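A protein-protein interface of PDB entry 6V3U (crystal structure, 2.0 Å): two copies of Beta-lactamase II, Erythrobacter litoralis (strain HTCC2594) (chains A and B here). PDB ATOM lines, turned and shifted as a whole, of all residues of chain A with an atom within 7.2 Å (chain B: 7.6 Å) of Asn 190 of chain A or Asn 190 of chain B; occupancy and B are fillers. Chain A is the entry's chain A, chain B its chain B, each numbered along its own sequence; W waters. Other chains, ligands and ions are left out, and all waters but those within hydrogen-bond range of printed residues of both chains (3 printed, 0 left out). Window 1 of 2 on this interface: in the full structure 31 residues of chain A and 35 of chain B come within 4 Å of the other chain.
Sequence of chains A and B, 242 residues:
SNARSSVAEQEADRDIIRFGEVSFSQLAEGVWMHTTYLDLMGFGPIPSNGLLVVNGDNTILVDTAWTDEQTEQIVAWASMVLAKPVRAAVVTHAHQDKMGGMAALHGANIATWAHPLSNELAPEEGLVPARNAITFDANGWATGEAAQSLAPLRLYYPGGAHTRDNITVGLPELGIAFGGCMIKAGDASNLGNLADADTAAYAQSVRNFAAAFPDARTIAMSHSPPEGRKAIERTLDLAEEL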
ATOM      1  N   OCS A 181     -20.887  29.174 -11.797  1.00  0.00           N
ATOM      2  CA  OCS A 181     -21.262  27.741 -11.835  1.00  0.00           C
ATOM      3  CB  OCS A 181     -20.515  27.038 -10.711  1.00  0.00           C
ATOM      4  SG  OCS A 181     -19.578  25.811 -11.315  1.00  0.00           S
ATOM      5  C   OCS A 181     -22.762  27.594 -11.747  1.00  0.00           C
ATOM      6  O   OCS A 181     -23.433  28.278 -10.976  1.00  0.00           O
ATOM      7  OD1 OCS A 181     -18.658  25.296 -10.269  1.00  0.00           O
ATOM      8  OD2 OCS A 181     -20.473  24.721 -11.762  1.00  0.00           O
ATOM      9  OD3 OCS A 181     -18.840  26.278 -12.505  1.00  0.00           O
ATOM     10  N   MET A 182     -23.307  26.718 -12.575  1.00  0.00           N
ATOM     11  CA  MET A 182     -24.741  26.489 -12.609  1.00  0.00           C
ATOM     12  C   MET A 182     -25.059  25.041 -12.315  1.00  0.00           C
ATOM     13  O   MET A 182     -24.188  24.180 -12.423  1.00  0.00           O
ATOM     14  CB  MET A 182     -25.314  26.887 -13.961  1.00  0.00           C
ATOM     15  CG  MET A 182     -25.676  28.341 -14.003  1.00  0.00           C
ATOM     16  SD  MET A 182     -26.302  28.858 -15.737  1.00  0.00           S
ATOM     17  CE  MET A 182     -24.633  29.614 -16.401  1.00  0.00           C
ATOM     18  N   ILE A 183     -26.315  24.791 -11.921  1.00  0.00           N
ATOM     19  CA  ILE A 183     -26.749  23.447 -11.571  1.00  0.00           C
ATOM     20  C   ILE A 183     -26.534  22.513 -12.746  1.00  0.00           C
ATOM     21  O   ILE A 183     -26.784  22.881 -13.900  1.00  0.00           O
ATOM     22  CB  ILE A 183     -28.231  23.464 -11.160  1.00  0.00           C
ATOM     23  CG1 ILE A 183     -28.463  24.486 -10.047  1.00  0.00           C
ATOM     24  CG2 ILE A 183     -28.676  22.073 -10.700  1.00  0.00           C
ATOM     25  CD1 ILE A 183     -27.848  24.074  -8.743  1.00  0.00           C
ATOM     26  N   LYS A 184     -26.079  21.293 -12.457  1.00  0.00           N
ATOM     27  CA  LYS A 184     -25.920  20.247 -13.458  1.00  0.00           C
ATOM     28  C   LYS A 184     -27.211  19.447 -13.620  1.00  0.00           C
ATOM     29  O   LYS A 184     -28.047  19.371 -12.710  1.00  0.00           O
ATOM     30  CB  LYS A 184     -24.775  19.308 -13.083  1.00  0.00           C
ATOM     31  CG  LYS A 184     -23.479  20.027 -12.784  1.00  0.00           C
ATOM     32  CD  LYS A 184     -23.088  20.927 -13.937  1.00  0.00           C
ATOM     33  CE  LYS A 184     -21.749  21.595 -13.675  1.00  0.00           C
ATOM     34  NZ  LYS A 184     -21.859  22.939 -13.031  1.00  0.00           N
ATOM     35  N   ASP A 187     -28.224  16.594 -11.010  1.00  0.00           N
ATOM     36  CA  ASP A 187     -27.451  16.787  -9.788  1.00  0.00           C
ATOM     37  C   ASP A 187     -28.319  17.473  -8.738  1.00  0.00           C
ATOM     38  O   ASP A 187     -28.727  18.625  -8.922  1.00  0.00           O
ATOM     39  CB  ASP A 187     -26.203  17.626 -10.073  1.00  0.00           C
ATOM     40  CG  ASP A 187     -25.210  17.620  -8.921  1.00  0.00           C
ATOM     41  OD1 ASP A 187     -24.094  18.158  -9.104  1.00  0.00           O
ATOM     42  OD2 ASP A 187     -25.542  17.062  -7.848  1.00  0.00           O
ATOM     43  N   ALA A 188     -28.585  16.778  -7.634  1.00  0.00           N
ATOM     44  CA  ALA A 188     -29.376  17.343  -6.554  1.00  0.00           C
ATOM     45  C   ALA A 188     -28.516  17.958  -5.459  1.00  0.00           C
ATOM     46  O   ALA A 188     -29.062  18.483  -4.484  1.00  0.00           O
ATOM     47  CB  ALA A 188     -30.285  16.266  -5.948  1.00  0.00           C
ATOM     48  N   SER A 189     -27.188  17.906  -5.603  1.00  0.00           N
ATOM     49  CA  SER A 189     -26.282  18.302  -4.524  1.00  0.00           C
ATOM     50  C   SER A 189     -26.574  19.707  -4.020  1.00  0.00           C
ATOM     51  O   SER A 189     -26.579  19.951  -2.809  1.00  0.00           O
ATOM     52  CB  SER A 189     -24.833  18.223  -5.002  1.00  0.00           C
ATOM     53  OG  SER A 189     -24.513  16.925  -5.485  1.00  0.00           O
ATOM     54  N   ASN A 190     -26.814  20.642  -4.933  1.00  0.00           N
ATOM     55  CA  ASN A 190     -26.956  22.052  -4.604  1.00  0.00           C
ATOM     56  C   ASN A 190     -28.408  22.470  -4.394  1.00  0.00           C
ATOM     57  O   ASN A 190     -28.673  23.660  -4.193  1.00  0.00           O
ATOM     58  CB  ASN A 190     -26.327  22.896  -5.713  1.00  0.00           C
ATOM     59  CG  ASN A 190     -25.797  24.225  -5.211  1.00  0.00           C
ATOM     60  OD1 ASN A 190     -25.788  25.223  -5.941  1.00  0.00           O
ATOM     61  ND2 ASN A 190     -25.356  24.247  -3.959  1.00  0.00           N
ATOM     62  N   LEU A 191     -29.352  21.525  -4.435  1.00  0.00           N
ATOM     63  CA  LEU A 191     -30.760  21.902  -4.488  1.00  0.00           C
ATOM     64  C   LEU A 191     -31.232  22.489  -3.161  1.00  0.00           C
ATOM     65  O   LEU A 191     -31.945  23.499  -3.140  1.00  0.00           O
ATOM     66  CB  LEU A 191     -31.610  20.696  -4.894  1.00  0.00           C
ATOM     67  CG  LEU A 191     -31.925  20.591  -6.387  1.00  0.00           C
ATOM     68  CD1 LEU A 191     -32.518  19.238  -6.747  1.00  0.00           C
ATOM     69  CD2 LEU A 191     -32.881  21.704  -6.777  1.00  0.00           C
ATOM     70  N   GLY A 192     -30.860  21.860  -2.043  1.00  0.00           N
ATOM     71  CA  GLY A 192     -31.226  22.406  -0.743  1.00  0.00           C
ATOM     72  C   GLY A 192     -30.597  23.764  -0.483  1.00  0.00           C
ATOM     73  O   GLY A 192     -31.244  24.673   0.039  1.00  0.00           O
ATOM     74  N   ASN A 193     -29.326  23.928  -0.852  1.00  0.00           N
ATOM     75  CA  ASN A 193     -28.718  25.249  -0.722  1.00  0.00           C
ATOM     76  C   ASN A 193     -29.501  26.299  -1.514  1.00  0.00           C
ATOM     77  O   ASN A 193     -29.664  27.436  -1.049  1.00  0.00           O
ATOM     78  CB  ASN A 193     -27.254  25.197  -1.164  1.00  0.00           C
ATOM     79  CG  ASN A 193     -26.377  24.413  -0.199  1.00  0.00           C
ATOM     80  OD1 ASN A 193     -26.538  24.496   1.017  1.00  0.00           O
ATOM     81  ND2 ASN A 193     -25.438  23.650  -0.745  1.00  0.00           N
ATOM     82  N   LEU A 194     -30.033  25.918  -2.683  1.00  0.00           N
ATOM     83  CA  LEU A 194     -30.790  26.840  -3.527  1.00  0.00           C
ATOM     84  C   LEU A 194     -32.135  27.212  -2.898  1.00  0.00           C
ATOM     85  O   LEU A 194     -32.579  28.361  -3.015  1.00  0.00           O
ATOM     86  CB  LEU A 194     -30.986  26.221  -4.922  1.00  0.00           C
ATOM     87  CG  LEU A 194     -31.814  26.993  -5.970  1.00  0.00           C
ATOM     88  CD1 LEU A 194     -31.191  28.353  -6.253  1.00  0.00           C
ATOM     89  CD2 LEU A 194     -32.008  26.228  -7.287  1.00  0.00           C
ATOM     90  N   ALA A 195     -32.812  26.265  -2.227  1.00  0.00           N
ATOM     91  CA  ALA A 195     -34.098  26.607  -1.626  1.00  0.00           C
ATOM     92  C   ALA A 195     -33.929  27.490  -0.396  1.00  0.00           C
ATOM     93  O   ALA A 195     -34.859  28.216  -0.012  1.00  0.00           O
ATOM     94  CB  ALA A 195     -34.888  25.338  -1.253  1.00  0.00           C
ATOM     95  N   ASP A 196     -32.777  27.411   0.259  1.00  0.00           N
ATOM     96  CA  ASP A 196     -32.555  28.133   1.505  1.00  0.00           C
ATOM     97  C   ASP A 196     -31.824  29.447   1.277  1.00  0.00           C
ATOM     98  O   ASP A 196     -31.494  30.143   2.235  1.00  0.00           O
ATOM     99  CB  ASP A 196     -31.805  27.246   2.501  1.00  0.00           C
ATOM    100  CG  ASP A 196     -32.606  26.027   2.884  1.00  0.00           C
ATOM    101  OD1 ASP A 196     -33.790  25.988   2.482  1.00  0.00           O
ATOM    102  OD2 ASP A 196     -32.083  25.126   3.581  1.00  0.00           O
ATOM    103  N   TYR A 202     -31.240  35.126  -6.907  1.00  0.00           N
ATOM    104  CA  TYR A 202     -30.463  34.277  -7.800  1.00  0.00           C
ATOM    105  C   TYR A 202     -31.142  34.158  -9.154  1.00  0.00           C
ATOM    106  O   TYR A 202     -30.488  34.274 -10.197  1.00  0.00           O
ATOM    107  CB  TYR A 202     -30.251  32.889  -7.191  1.00  0.00           C
ATOM    108  CG  TYR A 202     -29.317  32.020  -8.034  1.00  0.00           C
ATOM    109  CD1 TYR A 202     -27.968  32.343  -8.169  1.00  0.00           C
ATOM    110  CD2 TYR A 202     -29.784  30.881  -8.701  1.00  0.00           C
ATOM    111  CE1 TYR A 202     -27.106  31.562  -8.953  1.00  0.00           C
ATOM    112  CE2 TYR A 202     -28.924  30.088  -9.481  1.00  0.00           C
ATOM    113  CZ  TYR A 202     -27.587  30.433  -9.600  1.00  0.00           C
ATOM    114  OH  TYR A 202     -26.733  29.657 -10.369  1.00  0.00           O
ATOM    115  N   LEU A 242     -38.924  26.524  -6.487  1.00  0.00           N
ATOM    116  CA  LEU A 242     -38.422  26.741  -5.136  1.00  0.00           C
ATOM    117  C   LEU A 242     -38.620  28.198  -4.717  1.00  0.00           C
ATOM    118  O   LEU A 242     -38.002  28.672  -3.759  1.00  0.00           O
ATOM    119  CB  LEU A 242     -36.944  26.368  -5.047  1.00  0.00           C
ATOM    120  CG  LEU A 242     -36.594  24.942  -5.470  1.00  0.00           C
ATOM    121  CD1 LEU A 242     -35.080  24.806  -5.692  1.00  0.00           C
ATOM    122  CD2 LEU A 242     -37.107  23.947  -4.440  1.00  0.00           C
ATOM    123  N   PHE B  43     -34.660  15.721 -11.374  1.00  0.00           N
ATOM    124  CA  PHE B  43     -33.801  15.637 -10.199  1.00  0.00           C
ATOM    125  C   PHE B  43     -34.258  14.623  -9.163  1.00  0.00           C
ATOM    126  O   PHE B  43     -33.520  14.378  -8.201  1.00  0.00           O
ATOM    127  CB  PHE B  43     -33.677  17.009  -9.517  1.00  0.00           C
ATOM    128  CG  PHE B  43     -32.949  18.019 -10.342  1.00  0.00           C
ATOM    129  CD1 PHE B  43     -33.642  18.892 -11.160  1.00  0.00           C
ATOM    130  CD2 PHE B  43     -31.565  18.078 -10.325  1.00  0.00           C
ATOM    131  CE1 PHE B  43     -32.964  19.822 -11.946  1.00  0.00           C
ATOM    132  CE2 PHE B  43     -30.877  19.009 -11.112  1.00  0.00           C
ATOM    133  CZ  PHE B  43     -31.580  19.877 -11.918  1.00  0.00           C
ATOM    134  N   OCS B 181     -27.222  22.664   5.051  1.00  0.00           N
ATOM    135  CA  OCS B 181     -26.590  21.640   4.175  1.00  0.00           C
ATOM    136  CB  OCS B 181     -27.276  21.730   2.819  1.00  0.00           C
ATOM    137  SG  OCS B 181     -28.191  20.377   2.545  1.00  0.00           S
ATOM    138  C   OCS B 181     -25.091  21.799   4.058  1.00  0.00           C
ATOM    139  O   OCS B 181     -24.577  22.864   3.726  1.00  0.00           O
ATOM    140  OD1 OCS B 181     -27.277  19.267   2.215  1.00  0.00           O
ATOM    141  OD2 OCS B 181     -28.941  20.032   3.773  1.00  0.00           O
ATOM    142  OD3 OCS B 181     -29.111  20.571   1.402  1.00  0.00           O
ATOM    143  N   MET B 182     -24.365  20.729   4.348  1.00  0.00           N
ATOM    144  CA  MET B 182     -22.917  20.742   4.237  1.00  0.00           C
ATOM    145  C   MET B 182     -22.429  19.882   3.092  1.00  0.00           C
ATOM    146  O   MET B 182     -23.167  19.050   2.561  1.00  0.00           O
ATOM    147  CB  MET B 182     -22.274  20.265   5.527  1.00  0.00           C
ATOM    148  CG  MET B 182     -22.873  20.887   6.736  1.00  0.00           C
ATOM    149  SD  MET B 182     -21.650  20.692   8.198  1.00  0.00           S
ATOM    150  CE  MET B 182     -21.153  22.562   8.318  1.00  0.00           C
ATOM    151  N   ILE B 183     -21.161  20.103   2.730  1.00  0.00           N
ATOM    152  CA  ILE B 183     -20.546  19.382   1.628  1.00  0.00           C
ATOM    153  C   ILE B 183     -20.601  17.890   1.904  1.00  0.00           C
ATOM    154  O   ILE B 183     -20.204  17.429   2.982  1.00  0.00           O
ATOM    155  CB  ILE B 183     -19.099  19.856   1.431  1.00  0.00           C
ATOM    156  CG1 ILE B 183     -19.057  21.337   1.034  1.00  0.00           C
ATOM    157  CG2 ILE B 183     -18.406  18.999   0.385  1.00  0.00           C
ATOM    158  CD1 ILE B 183     -19.728  21.625  -0.285  1.00  0.00           C
ATOM    159  N   LYS B 184     -21.112  17.129   0.934  1.00  0.00           N
ATOM    160  CA  LYS B 184     -21.141  15.679   1.033  1.00  0.00           C
ATOM    161  C   LYS B 184     -19.759  15.088   0.787  1.00  0.00           C
ATOM    162  O   LYS B 184     -18.890  15.695   0.145  1.00  0.00           O
ATOM    163  CB  LYS B 184     -22.119  15.074   0.034  1.00  0.00           C
ATOM    164  CG  LYS B 184     -23.458  14.722   0.623  1.00  0.00           C
ATOM    165  CD  LYS B 184     -24.354  15.924   0.666  1.00  0.00           C
ATOM    166  CE  LYS B 184     -24.809  16.213   2.072  1.00  0.00           C
ATOM    167  NZ  LYS B 184     -25.669  17.434   2.114  1.00  0.00           N
ATOM    168  N   ASP B 187     -18.192  14.574  -3.043  1.00  0.00           N
ATOM    169  CA  ASP B 187     -18.989  15.303  -4.028  1.00  0.00           C
ATOM    170  C   ASP B 187     -18.348  16.663  -4.292  1.00  0.00           C
ATOM    171  O   ASP B 187     -18.360  17.541  -3.425  1.00  0.00           O
ATOM    172  CB  ASP B 187     -20.423  15.460  -3.526  1.00  0.00           C
ATOM    173  CG  ASP B 187     -21.352  16.046  -4.571  1.00  0.00           C
ATOM    174  OD1 ASP B 187     -20.963  16.113  -5.759  1.00  0.00           O
ATOM    175  OD2 ASP B 187     -22.476  16.436  -4.184  1.00  0.00           O
ATOM    176  N   ALA B 188     -17.802  16.847  -5.495  1.00  0.00           N
ATOM    177  CA  ALA B 188     -17.171  18.113  -5.845  1.00  0.00           C
ATOM    178  C   ALA B 188     -18.171  19.117  -6.450  1.00  0.00           C
ATOM    179  O   ALA B 188     -17.758  20.175  -6.922  1.00  0.00           O
ATOM    180  CB  ALA B 188     -16.014  17.876  -6.816  1.00  0.00           C
ATOM    181  N   SER B 189     -19.462  18.772  -6.403  1.00  0.00           N
ATOM    182  CA  SER B 189     -20.493  19.539  -7.103  1.00  0.00           C
ATOM    183  C   SER B 189     -20.485  21.007  -6.694  1.00  0.00           C
ATOM    184  O   SER B 189     -20.479  21.900  -7.550  1.00  0.00           O
ATOM    185  CB  SER B 189     -21.870  18.923  -6.836  1.00  0.00           C
ATOM    186  OG  SER B 189     -22.017  17.672  -7.491  1.00  0.00           O
ATOM    187  N   ASN B 190     -20.502  21.277  -5.389  1.00  0.00           N
ATOM    188  CA  ASN B 190     -20.592  22.639  -4.878  1.00  0.00           C
ATOM    189  C   ASN B 190     -19.228  23.241  -4.540  1.00  0.00           C
ATOM    190  O   ASN B 190     -19.174  24.302  -3.908  1.00  0.00           O
ATOM    191  CB  ASN B 190     -21.499  22.682  -3.641  1.00  0.00           C
ATOM    192  CG  ASN B 190     -22.877  22.083  -3.903  1.00  0.00           C
ATOM    193  OD1 ASN B 190     -23.355  22.065  -5.045  1.00  0.00           O
ATOM    194  ND2 ASN B 190     -23.522  21.591  -2.847  1.00  0.00           N
ATOM    195  N   LEU B 191     -18.127  22.591  -4.935  1.00  0.00           N
ATOM    196  CA  LEU B 191     -16.815  23.112  -4.569  1.00  0.00           C
ATOM    197  C   LEU B 191     -16.531  24.434  -5.269  1.00  0.00           C
ATOM    198  O   LEU B 191     -16.007  25.365  -4.649  1.00  0.00           O
ATOM    199  CB  LEU B 191     -15.721  22.091  -4.876  1.00  0.00           C
ATOM    200  CG  LEU B 191     -15.706  20.816  -4.024  1.00  0.00           C
ATOM    201  CD1 LEU B 191     -14.395  20.054  -4.234  1.00  0.00           C
ATOM    202  CD2 LEU B 191     -15.920  21.134  -2.559  1.00  0.00           C
ATOM    203  N   GLY B 192     -16.891  24.547  -6.548  1.00  0.00           N
ATOM    204  CA  GLY B 192     -16.620  25.779  -7.274  1.00  0.00           C
ATOM    205  C   GLY B 192     -17.405  26.957  -6.726  1.00  0.00           C
ATOM    206  O   GLY B 192     -16.888  28.072  -6.633  1.00  0.00           O
ATOM    207  N   ASN B 193     -18.665  26.730  -6.352  1.00  0.00           N
ATOM    208  CA  ASN B 193     -19.427  27.789  -5.699  1.00  0.00           C
ATOM    209  C   ASN B 193     -18.761  28.210  -4.394  1.00  0.00           C
ATOM    210  O   ASN B 193     -18.734  29.398  -4.054  1.00  0.00           O
ATOM    211  CB  ASN B 193     -20.861  27.328  -5.450  1.00  0.00           C
ATOM    212  CG  ASN B 193     -21.646  27.158  -6.732  1.00  0.00           C
ATOM    213  OD1 ASN B 193     -21.443  27.884  -7.701  1.00  0.00           O
ATOM    214  ND2 ASN B 193     -22.562  26.195  -6.740  1.00  0.00           N
ATOM    215  N   LEU B 194     -18.204  27.244  -3.663  1.00  0.00           N
ATOM    216  CA  LEU B 194     -17.546  27.533  -2.395  1.00  0.00           C
ATOM    217  C   LEU B 194     -16.311  28.402  -2.604  1.00  0.00           C
ATOM    218  O   LEU B 194     -16.081  29.359  -1.852  1.00  0.00           O
ATOM    219  CB  LEU B 194     -17.189  26.213  -1.700  1.00  0.00           C
ATOM    220  CG  LEU B 194     -16.520  26.181  -0.321  1.00  0.00           C
ATOM    221  CD1 LEU B 194     -17.365  26.855   0.749  1.00  0.00           C
ATOM    222  CD2 LEU B 194     -16.200  24.755   0.101  1.00  0.00           C
ATOM    223  N   ALA B 195     -15.510  28.094  -3.637  1.00  0.00           N
ATOM    224  CA  ALA B 195     -14.306  28.871  -3.901  1.00  0.00           C
ATOM    225  C   ALA B 195     -14.637  30.310  -4.276  1.00  0.00           C
ATOM    226  O   ALA B 195     -13.853  31.226  -3.996  1.00  0.00           O
ATOM    227  CB  ALA B 195     -13.485  28.217  -5.023  1.00  0.00           C
ATOM    228  N   ASP B 196     -15.779  30.530  -4.911  1.00  0.00           N
ATOM    229  CA  ASP B 196     -16.114  31.849  -5.423  1.00  0.00           C
ATOM    230  C   ASP B 196     -16.945  32.667  -4.448  1.00  0.00           C
ATOM    231  O   ASP B 196     -17.226  33.838  -4.718  1.00  0.00           O
ATOM    232  CB  ASP B 196     -16.839  31.714  -6.765  1.00  0.00           C
ATOM    233  CG  ASP B 196     -15.915  31.235  -7.868  1.00  0.00           C
ATOM    234  OD1 ASP B 196     -14.695  31.143  -7.602  1.00  0.00           O
ATOM    235  OD2 ASP B 196     -16.403  30.948  -8.983  1.00  0.00           O
ATOM    236  N   LEU B 238     -11.926  22.052   3.517  1.00  0.00           N
ATOM    237  CA  LEU B 238     -12.058  22.663   2.199  1.00  0.00           C
ATOM    238  C   LEU B 238     -11.867  24.174   2.258  1.00  0.00           C
ATOM    239  O   LEU B 238     -11.204  24.751   1.388  1.00  0.00           O
ATOM    240  CB  LEU B 238     -13.411  22.305   1.591  1.00  0.00           C
ATOM    241  CG  LEU B 238     -13.468  20.881   1.035  1.00  0.00           C
ATOM    242  CD1 LEU B 238     -14.904  20.405   0.924  1.00  0.00           C
ATOM    243  CD2 LEU B 238     -12.757  20.793  -0.317  1.00  0.00           C
ATOM    244  N   LEU B 242      -9.065  26.151  -0.035  1.00  0.00           N
ATOM    245  CA  LEU B 242      -9.402  27.064  -1.128  1.00  0.00           C
ATOM    246  C   LEU B 242     -10.191  28.270  -0.620  1.00  0.00           C
ATOM    247  O   LEU B 242      -9.651  29.140   0.062  1.00  0.00           O
ATOM    248  CB  LEU B 242     -10.195  26.344  -2.226  1.00  0.00           C
ATOM    249  CG  LEU B 242     -11.352  25.397  -1.882  1.00  0.00           C
ATOM    250  CD1 LEU B 242     -12.571  26.097  -1.277  1.00  0.00           C
ATOM    251  CD2 LEU B 242     -11.753  24.620  -3.121  1.00  0.00           C
HETATM  252  O   HOH W   1     -23.247  23.786   1.338  1.00  0.00           O
HETATM  253  O   HOH W   2     -24.607  26.804  -8.731  1.00  0.00           O
HETATM  254  O   HOH W   3     -29.479  24.638   3.902  1.00  0.00           O
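OD1 of Asn 190 of chain B is in hydrogen-bond range of ND2 of Asn 190 of chain A. The side-chain carboxylate of Asp 187 of chain B sits at hydrogen-bond distance from the side-chain hydroxyl of Ser 189 of chain A (2.5 Å). OD1 of Asn 190 of chain A sits at hydrogen-bond distance from ND2 of Asn 193 of chain B (3.5 Å). OG of Ser 189 of chain A lies within hydrogen-bond range of OG of Ser 189 of chain B (3.3 Å). The side-chain hydroxyl of Ser 189 of chain B lies within hydrogen-bond range of the side-chain carboxylate of Asp 187 of chain A, at 2.7 Å. O of Ser 189 of chain A lies within hydrogen-bond range of ND2 of Asn 190 of chain B.
The side-chain amino group (NZ) of Lys 184 of chain A sits at hydrogen-bond distance from the backbone carbonyl oxygen (O) of Met 182 of chain A (2.7 Å). The side-chain carboxylate (OD1) of Asp 187 of chain B sits at hydrogen-bond distance from the side-chain hydroxyl (OG) of Ser 189 of chain B (2.6 Å). OD1 of OCS 181 of chain B lies close to the side-chain amino group (NZ) of Lys 184 of chain B (2.4 Å). OD2 of OCS 181 of chain A lies close to NZ of Lys 184 of chain A (2.6 Å). OG of Ser 189 of chain A lies within hydrogen-bond range of OD2 of Asp 187 of chain A. The side-chain amide nitrogen (ND2) of Asn 190 of chain A sits close to the side-chain amide nitrogen (ND2) of Asn 193 of chain A, at 3.3 Å.
OD1 of OCS 181 of chain A touches CA of Gly 192 of chain B, at 3.7 Å. Asn 193 of chain B touches OCS 181 of chain A (OD1 to CB, 3.3 Å). CE2 of Phe 43 of chain B touches CG2 of Ile 183 of chain A, at 3.8 Å. Lys 184 of chain A touches Phe 43 of chain B (O to CE2, 3.3 Å). Phe 43 of chain B touches Asp 187 of chain A. Phe 43 of chain B touches Leu 191 of chain A (CB to CD1, 3.7 Å). Gly 192 of chain A touches OCS 181 of chain B. CB of OCS 181 of chain B touches OD1 of Asn 193 of chain A, at 3.4 Å. Asn 190 of chain B touches Asn 193 of chain A.
Printed residues of chain B within 4 Å of Asn 190 of chain A: Asn 190 and Asn 193. Of chain A, only Ser 189, Asn 190 and Asn 193 come within 4 Å of Asn 190 of chain B. Printed residues of chain B within 4 Å of Leu 191 of chain A: Phe 43 (3.7 Å). Of the printed residues of chain A, Phe 43 of chain B touches Ile 183 (3.8 Å), Lys 184 (3.3 Å), Asp 187 (3.1 Å) and Leu 191 (3.7 Å). Of the printed residues of chain B, Asn 193 of chain A touches OCS 181 (3.4 Å) and Asn 190 (3.5 Å). Asp 196 of chain B touches none of the printed residues of chain A. Met 182 of chain A touches none of the printed residues of chain B. The nearest residue of chain B that does not touch Asn 190 of chain A is Ser 189 of chain B (5.6 Å).
Printed residues of chain B that touch a printed residue of chain A: Phe 43, OCS 181, Asp 187, Ser 189, Asn 190, Gly 192 and Asn 193. Hydrophobic or aromatic side chains of chain B that line the printed part of chain A: Phe 43. Among the printed residues, 15 pairs touch across the chains. Among the printed residues, no Asp or Glu carboxylate lies within 4 Å of a Lys or Arg side-chain nitrogen of the other chain.
OCS 181 of chain A touches Asn 193 of chain B, and with the chains exchanged Asn 193 of chain A touches OCS 181 of chain B. Asp 187 of chain A touches Ser 189 of chain B, and with the chains exchanged Ser 189 of chain A touches Asp 187 of chain B. Ser 189 of chain A touches Asn 190 of chain B, but with the chains exchanged Asn 190 of chain A does not touch Ser 189 of chain B (5.6 Å). Asn 190 of chain A touches Asn 193 of chain B, and with the chains exchanged Asn 193 of chain A touches Asn 190 of chain B.
Water W3 bridges the side-chain carboxylate of Asp 196 of chain A (2.7 Å) and N of OCS 181 of chain B (3.2 Å). Water W1 lies within hydrogen-bond range of O of OCS 181 of chain B (2.9 Å) and ND2 of Asn 193 of chain A (3.0 Å). Water W2 lies within hydrogen-bond range of ND2 of Asn 193 of chain B (2.9 Å), O of OCS 181 of chain A (2.9 Å) and OD1 of Asn 190 of chain A (3.4 Å).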
